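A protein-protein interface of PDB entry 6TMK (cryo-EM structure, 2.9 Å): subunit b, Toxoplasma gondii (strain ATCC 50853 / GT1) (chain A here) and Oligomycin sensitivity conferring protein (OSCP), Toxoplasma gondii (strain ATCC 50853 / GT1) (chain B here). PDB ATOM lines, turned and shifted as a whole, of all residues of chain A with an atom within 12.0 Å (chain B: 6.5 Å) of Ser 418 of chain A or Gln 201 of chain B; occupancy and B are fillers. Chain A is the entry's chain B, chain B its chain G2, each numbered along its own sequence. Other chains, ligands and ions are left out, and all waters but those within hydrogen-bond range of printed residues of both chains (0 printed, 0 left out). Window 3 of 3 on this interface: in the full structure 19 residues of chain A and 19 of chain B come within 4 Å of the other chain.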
ATOM      1  N   ALA A 409     -29.935  -7.218 -14.208  1.00  0.00           N
ATOM      2  CA  ALA A 409     -29.035  -6.124 -13.862  1.00  0.00           C
ATOM      3  C   ALA A 409     -27.769  -6.646 -13.197  1.00  0.00           C
ATOM      4  O   ALA A 409     -26.677  -6.105 -13.410  1.00  0.00           O
ATOM      5  CB  ALA A 409     -29.749  -5.127 -12.948  1.00  0.00           C
ATOM      6  N   MET A 410     -27.902  -7.680 -12.366  1.00  0.00           N
ATOM      7  CA  MET A 410     -26.729  -8.330 -11.789  1.00  0.00           C
ATOM      8  C   MET A 410     -25.776  -8.791 -12.888  1.00  0.00           C
ATOM      9  O   MET A 410     -24.584  -8.454 -12.884  1.00  0.00           O
ATOM     10  CB  MET A 410     -27.165  -9.506 -10.915  1.00  0.00           C
ATOM     11  CG  MET A 410     -26.059 -10.075 -10.035  1.00  0.00           C
ATOM     12  SD  MET A 410     -25.279  -8.867  -8.938  1.00  0.00           S
ATOM     13  CE  MET A 410     -26.693  -7.937  -8.347  1.00  0.00           C
ATOM     14  N   GLN A 411     -26.287  -9.594 -13.825  1.00  0.00           N
ATOM     15  CA  GLN A 411     -25.473 -10.059 -14.943  1.00  0.00           C
ATOM     16  C   GLN A 411     -24.907  -8.890 -15.737  1.00  0.00           C
ATOM     17  O   GLN A 411     -23.775  -8.955 -16.232  1.00  0.00           O
ATOM     18  CB  GLN A 411     -26.302 -10.971 -15.848  1.00  0.00           C
ATOM     19  CG  GLN A 411     -25.558 -11.490 -17.071  1.00  0.00           C
ATOM     20  CD  GLN A 411     -24.299 -12.256 -16.711  1.00  0.00           C
ATOM     21  OE1 GLN A 411     -24.308 -13.484 -16.626  1.00  0.00           O
ATOM     22  NE2 GLN A 411     -23.206 -11.530 -16.501  1.00  0.00           N
ATOM     23  N   SER A 412     -25.680  -7.811 -15.874  1.00  0.00           N
ATOM     24  CA  SER A 412     -25.217  -6.669 -16.651  1.00  0.00           C
ATOM     25  C   SER A 412     -24.001  -6.045 -15.986  1.00  0.00           C
ATOM     26  O   SER A 412     -22.994  -5.766 -16.643  1.00  0.00           O
ATOM     27  CB  SER A 412     -26.341  -5.644 -16.802  1.00  0.00           C
ATOM     28  OG  SER A 412     -26.416  -4.802 -15.665  1.00  0.00           O
ATOM     29  N   ALA A 413     -24.081  -5.816 -14.674  1.00  0.00           N
ATOM     30  CA  ALA A 413     -22.938  -5.275 -13.947  1.00  0.00           C
ATOM     31  C   ALA A 413     -21.744  -6.216 -14.047  1.00  0.00           C
ATOM     32  O   ALA A 413     -20.603  -5.777 -14.248  1.00  0.00           O
ATOM     33  CB  ALA A 413     -23.305  -5.045 -12.482  1.00  0.00           C
ATOM     34  N   ILE A 414     -21.989  -7.517 -13.883  1.00  0.00           N
ATOM     35  CA  ILE A 414     -20.898  -8.486 -13.917  1.00  0.00           C
ATOM     36  C   ILE A 414     -20.163  -8.408 -15.249  1.00  0.00           C
ATOM     37  O   ILE A 414     -18.935  -8.269 -15.294  1.00  0.00           O
ATOM     38  CB  ILE A 414     -21.433  -9.903 -13.647  1.00  0.00           C
ATOM     39  CG1 ILE A 414     -21.966 -10.005 -12.215  1.00  0.00           C
ATOM     40  CG2 ILE A 414     -20.343 -10.938 -13.882  1.00  0.00           C
ATOM     41  CD1 ILE A 414     -23.005 -11.084 -12.025  1.00  0.00           C
ATOM     42  N   GLN A 415     -20.904  -8.499 -16.357  1.00  0.00           N
ATOM     43  CA  GLN A 415     -20.279  -8.375 -17.669  1.00  0.00           C
ATOM     44  C   GLN A 415     -19.720  -6.982 -17.927  1.00  0.00           C
ATOM     45  O   GLN A 415     -18.828  -6.836 -18.770  1.00  0.00           O
ATOM     46  CB  GLN A 415     -21.290  -8.734 -18.759  1.00  0.00           C
ATOM     47  CG  GLN A 415     -20.690  -8.844 -20.152  1.00  0.00           C
ATOM     48  CD  GLN A 415     -20.802  -7.554 -20.942  1.00  0.00           C
ATOM     49  OE1 GLN A 415     -21.832  -6.880 -20.911  1.00  0.00           O
ATOM     50  NE2 GLN A 415     -19.740  -7.206 -21.660  1.00  0.00           N
ATOM     51  N   GLY A 416     -20.214  -5.957 -17.226  1.00  0.00           N
ATOM     52  CA  GLY A 416     -19.645  -4.628 -17.362  1.00  0.00           C
ATOM     53  C   GLY A 416     -18.349  -4.437 -16.615  1.00  0.00           C
ATOM     54  O   GLY A 416     -17.619  -3.479 -16.890  1.00  0.00           O
ATOM     55  N   LEU A 417     -18.046  -5.331 -15.674  1.00  0.00           N
ATOM     56  CA  LEU A 417     -16.780  -5.235 -14.953  1.00  0.00           C
ATOM     57  C   LEU A 417     -15.582  -5.639 -15.802  1.00  0.00           C
ATOM     58  O   LEU A 417     -14.465  -5.679 -15.275  1.00  0.00           O
ATOM     59  CB  LEU A 417     -16.807  -6.098 -13.690  1.00  0.00           C
ATOM     60  CG  LEU A 417     -17.847  -5.757 -12.625  1.00  0.00           C
ATOM     61  CD1 LEU A 417     -18.135  -6.973 -11.763  1.00  0.00           C
ATOM     62  CD2 LEU A 417     -17.369  -4.598 -11.772  1.00  0.00           C
ATOM     63  N   SER A 418     -15.776  -5.939 -17.084  1.00  0.00           N
ATOM     64  CA  SER A 418     -14.682  -6.350 -17.956  1.00  0.00           C
ATOM     65  C   SER A 418     -14.650  -5.497 -19.219  1.00  0.00           C
ATOM     66  O   SER A 418     -15.533  -4.669 -19.441  1.00  0.00           O
ATOM     67  CB  SER A 418     -14.818  -7.828 -18.325  1.00  0.00           C
ATOM     68  OG  SER A 418     -15.631  -7.992 -19.473  1.00  0.00           O
ATOM     69  N   MET A 424     -26.968  -5.310 -23.181  1.00  0.00           N
ATOM     70  CA  MET A 424     -27.085  -4.029 -22.496  1.00  0.00           C
ATOM     71  C   MET A 424     -27.941  -4.157 -21.241  1.00  0.00           C
ATOM     72  O   MET A 424     -28.757  -5.071 -21.125  1.00  0.00           O
ATOM     73  CB  MET A 424     -27.684  -2.976 -23.431  1.00  0.00           C
ATOM     74  CG  MET A 424     -27.680  -1.567 -22.859  1.00  0.00           C
ATOM     75  SD  MET A 424     -27.912  -0.304 -24.124  1.00  0.00           S
ATOM     76  CE  MET A 424     -26.961   1.045 -23.430  1.00  0.00           C
ATOM     77  N   ILE B 196     -16.568 -11.801  -7.654  1.00  0.00           N
ATOM     78  CA  ILE B 196     -15.173 -11.782  -7.230  1.00  0.00           C
ATOM     79  C   ILE B 196     -14.258 -12.052  -8.417  1.00  0.00           C
ATOM     80  O   ILE B 196     -13.212 -11.411  -8.563  1.00  0.00           O
ATOM     81  CB  ILE B 196     -14.932 -12.782  -6.084  1.00  0.00           C
ATOM     82  CG1 ILE B 196     -15.297 -14.203  -6.510  1.00  0.00           C
ATOM     83  CG2 ILE B 196     -15.727 -12.374  -4.852  1.00  0.00           C
ATOM     84  CD1 ILE B 196     -14.946 -15.254  -5.482  1.00  0.00           C
ATOM     85  N   VAL B 197     -14.647 -12.966  -9.309  1.00  0.00           N
ATOM     86  CA  VAL B 197     -13.776 -13.278 -10.437  1.00  0.00           C
ATOM     87  C   VAL B 197     -13.762 -12.123 -11.432  1.00  0.00           C
ATOM     88  O   VAL B 197     -12.722 -11.815 -12.031  1.00  0.00           O
ATOM     89  CB  VAL B 197     -14.204 -14.599 -11.103  1.00  0.00           C
ATOM     90  CG1 VAL B 197     -15.578 -14.467 -11.738  1.00  0.00           C
ATOM     91  CG2 VAL B 197     -13.173 -15.031 -12.134  1.00  0.00           C
ATOM     92  N   ALA B 198     -14.903 -11.450 -11.614  1.00  0.00           N
ATOM     93  CA  ALA B 198     -14.936 -10.301 -12.511  1.00  0.00           C
ATOM     94  C   ALA B 198     -14.095  -9.157 -11.962  1.00  0.00           C
ATOM     95  O   ALA B 198     -13.308  -8.546 -12.696  1.00  0.00           O
ATOM     96  CB  ALA B 198     -16.379  -9.850 -12.732  1.00  0.00           C
ATOM     97  N   ALA B 199     -14.222  -8.870 -10.664  1.00  0.00           N
ATOM     98  CA  ALA B 199     -13.401  -7.826 -10.069  1.00  0.00           C
ATOM     99  C   ALA B 199     -11.933  -8.216 -10.039  1.00  0.00           C
ATOM    100  O   ALA B 199     -11.070  -7.336 -10.096  1.00  0.00           O
ATOM    101  CB  ALA B 199     -13.888  -7.518  -8.655  1.00  0.00           C
ATOM    102  N   LEU B 200     -11.630  -9.514 -10.040  1.00  0.00           N
ATOM    103  CA  LEU B 200     -10.241  -9.944 -10.040  1.00  0.00           C
ATOM    104  C   LEU B 200      -9.626  -9.778 -11.422  1.00  0.00           C
ATOM    105  O   LEU B 200      -8.492  -9.305 -11.544  1.00  0.00           O
ATOM    106  CB  LEU B 200     -10.143 -11.398  -9.581  1.00  0.00           C
ATOM    107  CG  LEU B 200      -8.772 -12.072  -9.682  1.00  0.00           C
ATOM    108  CD1 LEU B 200      -7.670 -11.186  -9.114  1.00  0.00           C
ATOM    109  CD2 LEU B 200      -8.796 -13.414  -8.972  1.00  0.00           C
ATOM    110  N   GLN B 201     -10.351 -10.161 -12.474  1.00  0.00           N
ATOM    111  CA  GLN B 201      -9.838  -9.927 -13.819  1.00  0.00           C
ATOM    112  C   GLN B 201      -9.797  -8.437 -14.143  1.00  0.00           C
ATOM    113  O   GLN B 201      -8.999  -8.011 -14.987  1.00  0.00           O
ATOM    114  CB  GLN B 201     -10.677 -10.676 -14.859  1.00  0.00           C
ATOM    115  CG  GLN B 201     -12.174 -10.388 -14.821  1.00  0.00           C
ATOM    116  CD  GLN B 201     -12.545  -9.086 -15.513  1.00  0.00           C
ATOM    117  OE1 GLN B 201     -11.741  -8.507 -16.243  1.00  0.00           O
ATOM    118  NE2 GLN B 201     -13.767  -8.620 -15.283  1.00  0.00           N
ATOM    119  N   ASN B 202     -10.641  -7.632 -13.491  1.00  0.00           N
ATOM    120  CA  ASN B 202     -10.575  -6.184 -13.673  1.00  0.00           C
ATOM    121  C   ASN B 202      -9.353  -5.591 -12.976  1.00  0.00           C
ATOM    122  O   ASN B 202      -8.640  -4.761 -13.552  1.00  0.00           O
ATOM    123  CB  ASN B 202     -11.859  -5.538 -13.151  1.00  0.00           C
ATOM    124  CG  ASN B 202     -11.985  -4.081 -13.553  1.00  0.00           C
ATOM    125  OD1 ASN B 202     -11.084  -3.276 -13.312  1.00  0.00           O
ATOM    126  ND2 ASN B 202     -13.109  -3.733 -14.170  1.00  0.00           N
ATOM    127  N   ARG B 203      -9.098  -6.007 -11.735  1.00  0.00           N
ATOM    128  CA  ARG B 203      -7.950  -5.504 -10.988  1.00  0.00           C
ATOM    129  C   ARG B 203      -6.637  -5.960 -11.611  1.00  0.00           C
ATOM    130  O   ARG B 203      -5.714  -5.159 -11.800  1.00  0.00           O
ATOM    131  CB  ARG B 203      -8.030  -5.967  -9.533  1.00  0.00           C
ATOM    132  CG  ARG B 203      -8.815  -5.045  -8.620  1.00  0.00           C
ATOM    133  CD  ARG B 203      -9.001  -5.666  -7.244  1.00  0.00           C
ATOM    134  NE  ARG B 203      -7.726  -5.967  -6.598  1.00  0.00           N
ATOM    135  CZ  ARG B 203      -7.572  -6.165  -5.291  1.00  0.00           C
ATOM    136  NH1 ARG B 203      -8.614  -6.088  -4.473  1.00  0.00           N
ATOM    137  NH2 ARG B 203      -6.371  -6.435  -4.799  1.00  0.00           N
ATOM    138  N   ALA B 204      -6.536  -7.249 -11.930  1.00  0.00           N
ATOM    139  CA  ALA B 204      -5.262  -7.914 -12.183  1.00  0.00           C
ATOM    140  C   ALA B 204      -4.332  -7.787 -10.982  1.00  0.00           C
ATOM    141  O   ALA B 204      -3.107  -7.740 -11.127  1.00  0.00           O
ATOM    142  CB  ALA B 204      -4.586  -7.364 -13.442  1.00  0.00           C
ATOM    143  N   PHE B 235     -21.479   0.952 -10.726  1.00  0.00           N
ATOM    144  CA  PHE B 235     -22.403   0.015 -11.354  1.00  0.00           C
ATOM    145  C   PHE B 235     -23.655  -0.142 -10.502  1.00  0.00           C
ATOM    146  O   PHE B 235     -23.723  -1.025  -9.641  1.00  0.00           O
ATOM    147  CB  PHE B 235     -21.734  -1.347 -11.563  1.00  0.00           C
ATOM    148  CG  PHE B 235     -20.665  -1.352 -12.622  1.00  0.00           C
ATOM    149  CD1 PHE B 235     -20.283  -0.182 -13.261  1.00  0.00           C
ATOM    150  CD2 PHE B 235     -20.044  -2.536 -12.984  1.00  0.00           C
ATOM    151  CE1 PHE B 235     -19.303  -0.193 -14.232  1.00  0.00           C
ATOM    152  CE2 PHE B 235     -19.064  -2.554 -13.956  1.00  0.00           C
ATOM    153  CZ  PHE B 235     -18.693  -1.381 -14.581  1.00  0.00           C
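Phe 235 of chain B touches Ala 413 of chain A (CD2 to O, 3.5 Å).
Ile 414 of chain A touches Ala 198 of chain B.
Gly 416 of chain A touches Phe 235 of chain B.
Leu 417 of chain A touches Ala 198 of chain B (CD1 to CB, 3.5 Å).
N of Leu 417 of chain A touches CE2 of Phe 235 of chain B (3.4 Å).
Ser 418 of chain A touches Gln 201 of chain B.
OG of Ser 418 of chain A sits at hydrogen-bond distance from O of Gln 415 of chain A (3.5 Å).
The backbone carbonyl oxygen of Ala 198 of chain B sits at hydrogen-bond distance from the side-chain amide nitrogen of Gln 201 of chain B (2.6 Å).
Ser 412 of chain A touches none of the printed residues of chain B.
Printed residues of chain B within 4 Å of Ala 413 of chain A: Phe 235.
Of the printed residues of chain B, Ile 414 of chain A touches Ala 198 (3.9 Å).
Printed residues of chain B within 4 Å of Gly 416 of chain A: Phe 235.
Printed residues of chain B within 4 Å of Leu 417 of chain A: Ala 198 (3.5 Å), Gln 201 (3.0 Å), Asn 202 (2.6 Å) and Phe 235 (3.4 Å).
Ser 418 of chain A touches one residue of chain B.
No residue of chain A comes within 4 Å of Val 197 of chain B.
Ala 198 of chain B touches just these residues of chain A: Ile 414 and Leu 417.
No residue of chain A comes within 4 Å of Ala 199 of chain B.
No residue of chain A comes within 4 Å of Leu 200 of chain B.
Of chain A, only Leu 417 and Ser 418 come within 4 Å of Gln 201 of chain B.
Asn 202 of chain B touches just one residue of chain A: Leu 417.
No residue of chain A comes within 4 Å of Ala 204 of chain B.
Printed residues of chain A within 4 Å of Phe 235 of chain B: Ala 413 (3.5 Å), Gly 416 (3.3 Å) and Leu 417 (3.4 Å).
The nearest residue of chain B that does not touch Ser 418 of chain A is Asn 202 of chain B (4.5 Å).
The nearest residue of chain A that does not touch Gln 201 of chain B is Ile 414 of chain A (5.2 Å).
Hydrophobic or aromatic side chains of chain B within 4 Å of the printed part of chain A: Ala 198 and Phe 235.
Printed residues of chain A that touch a printed residue of chain B: Ala 413, Ile 414, Gly 416, Leu 417 and Ser 418.
Hydrophobic or aromatic side chains of chain A that line the printed part of chain B: Leu 417.
Among the printed residues, no Asp or Glu carboxylate lies within 4 Å of a Lys or Arg side-chain nitrogen of the other chain.
The side-chain amide nitrogen of Gln 201 of chain B is in hydrogen-bond range of the backbone carbonyl oxygen of Leu 417 of chain A.
The backbone carbonyl oxygen (O) of Leu 417 of chain A sits at hydrogen-bond distance from the side-chain amide nitrogen (ND2) of Asn 202 of chain B (2.6 Å).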
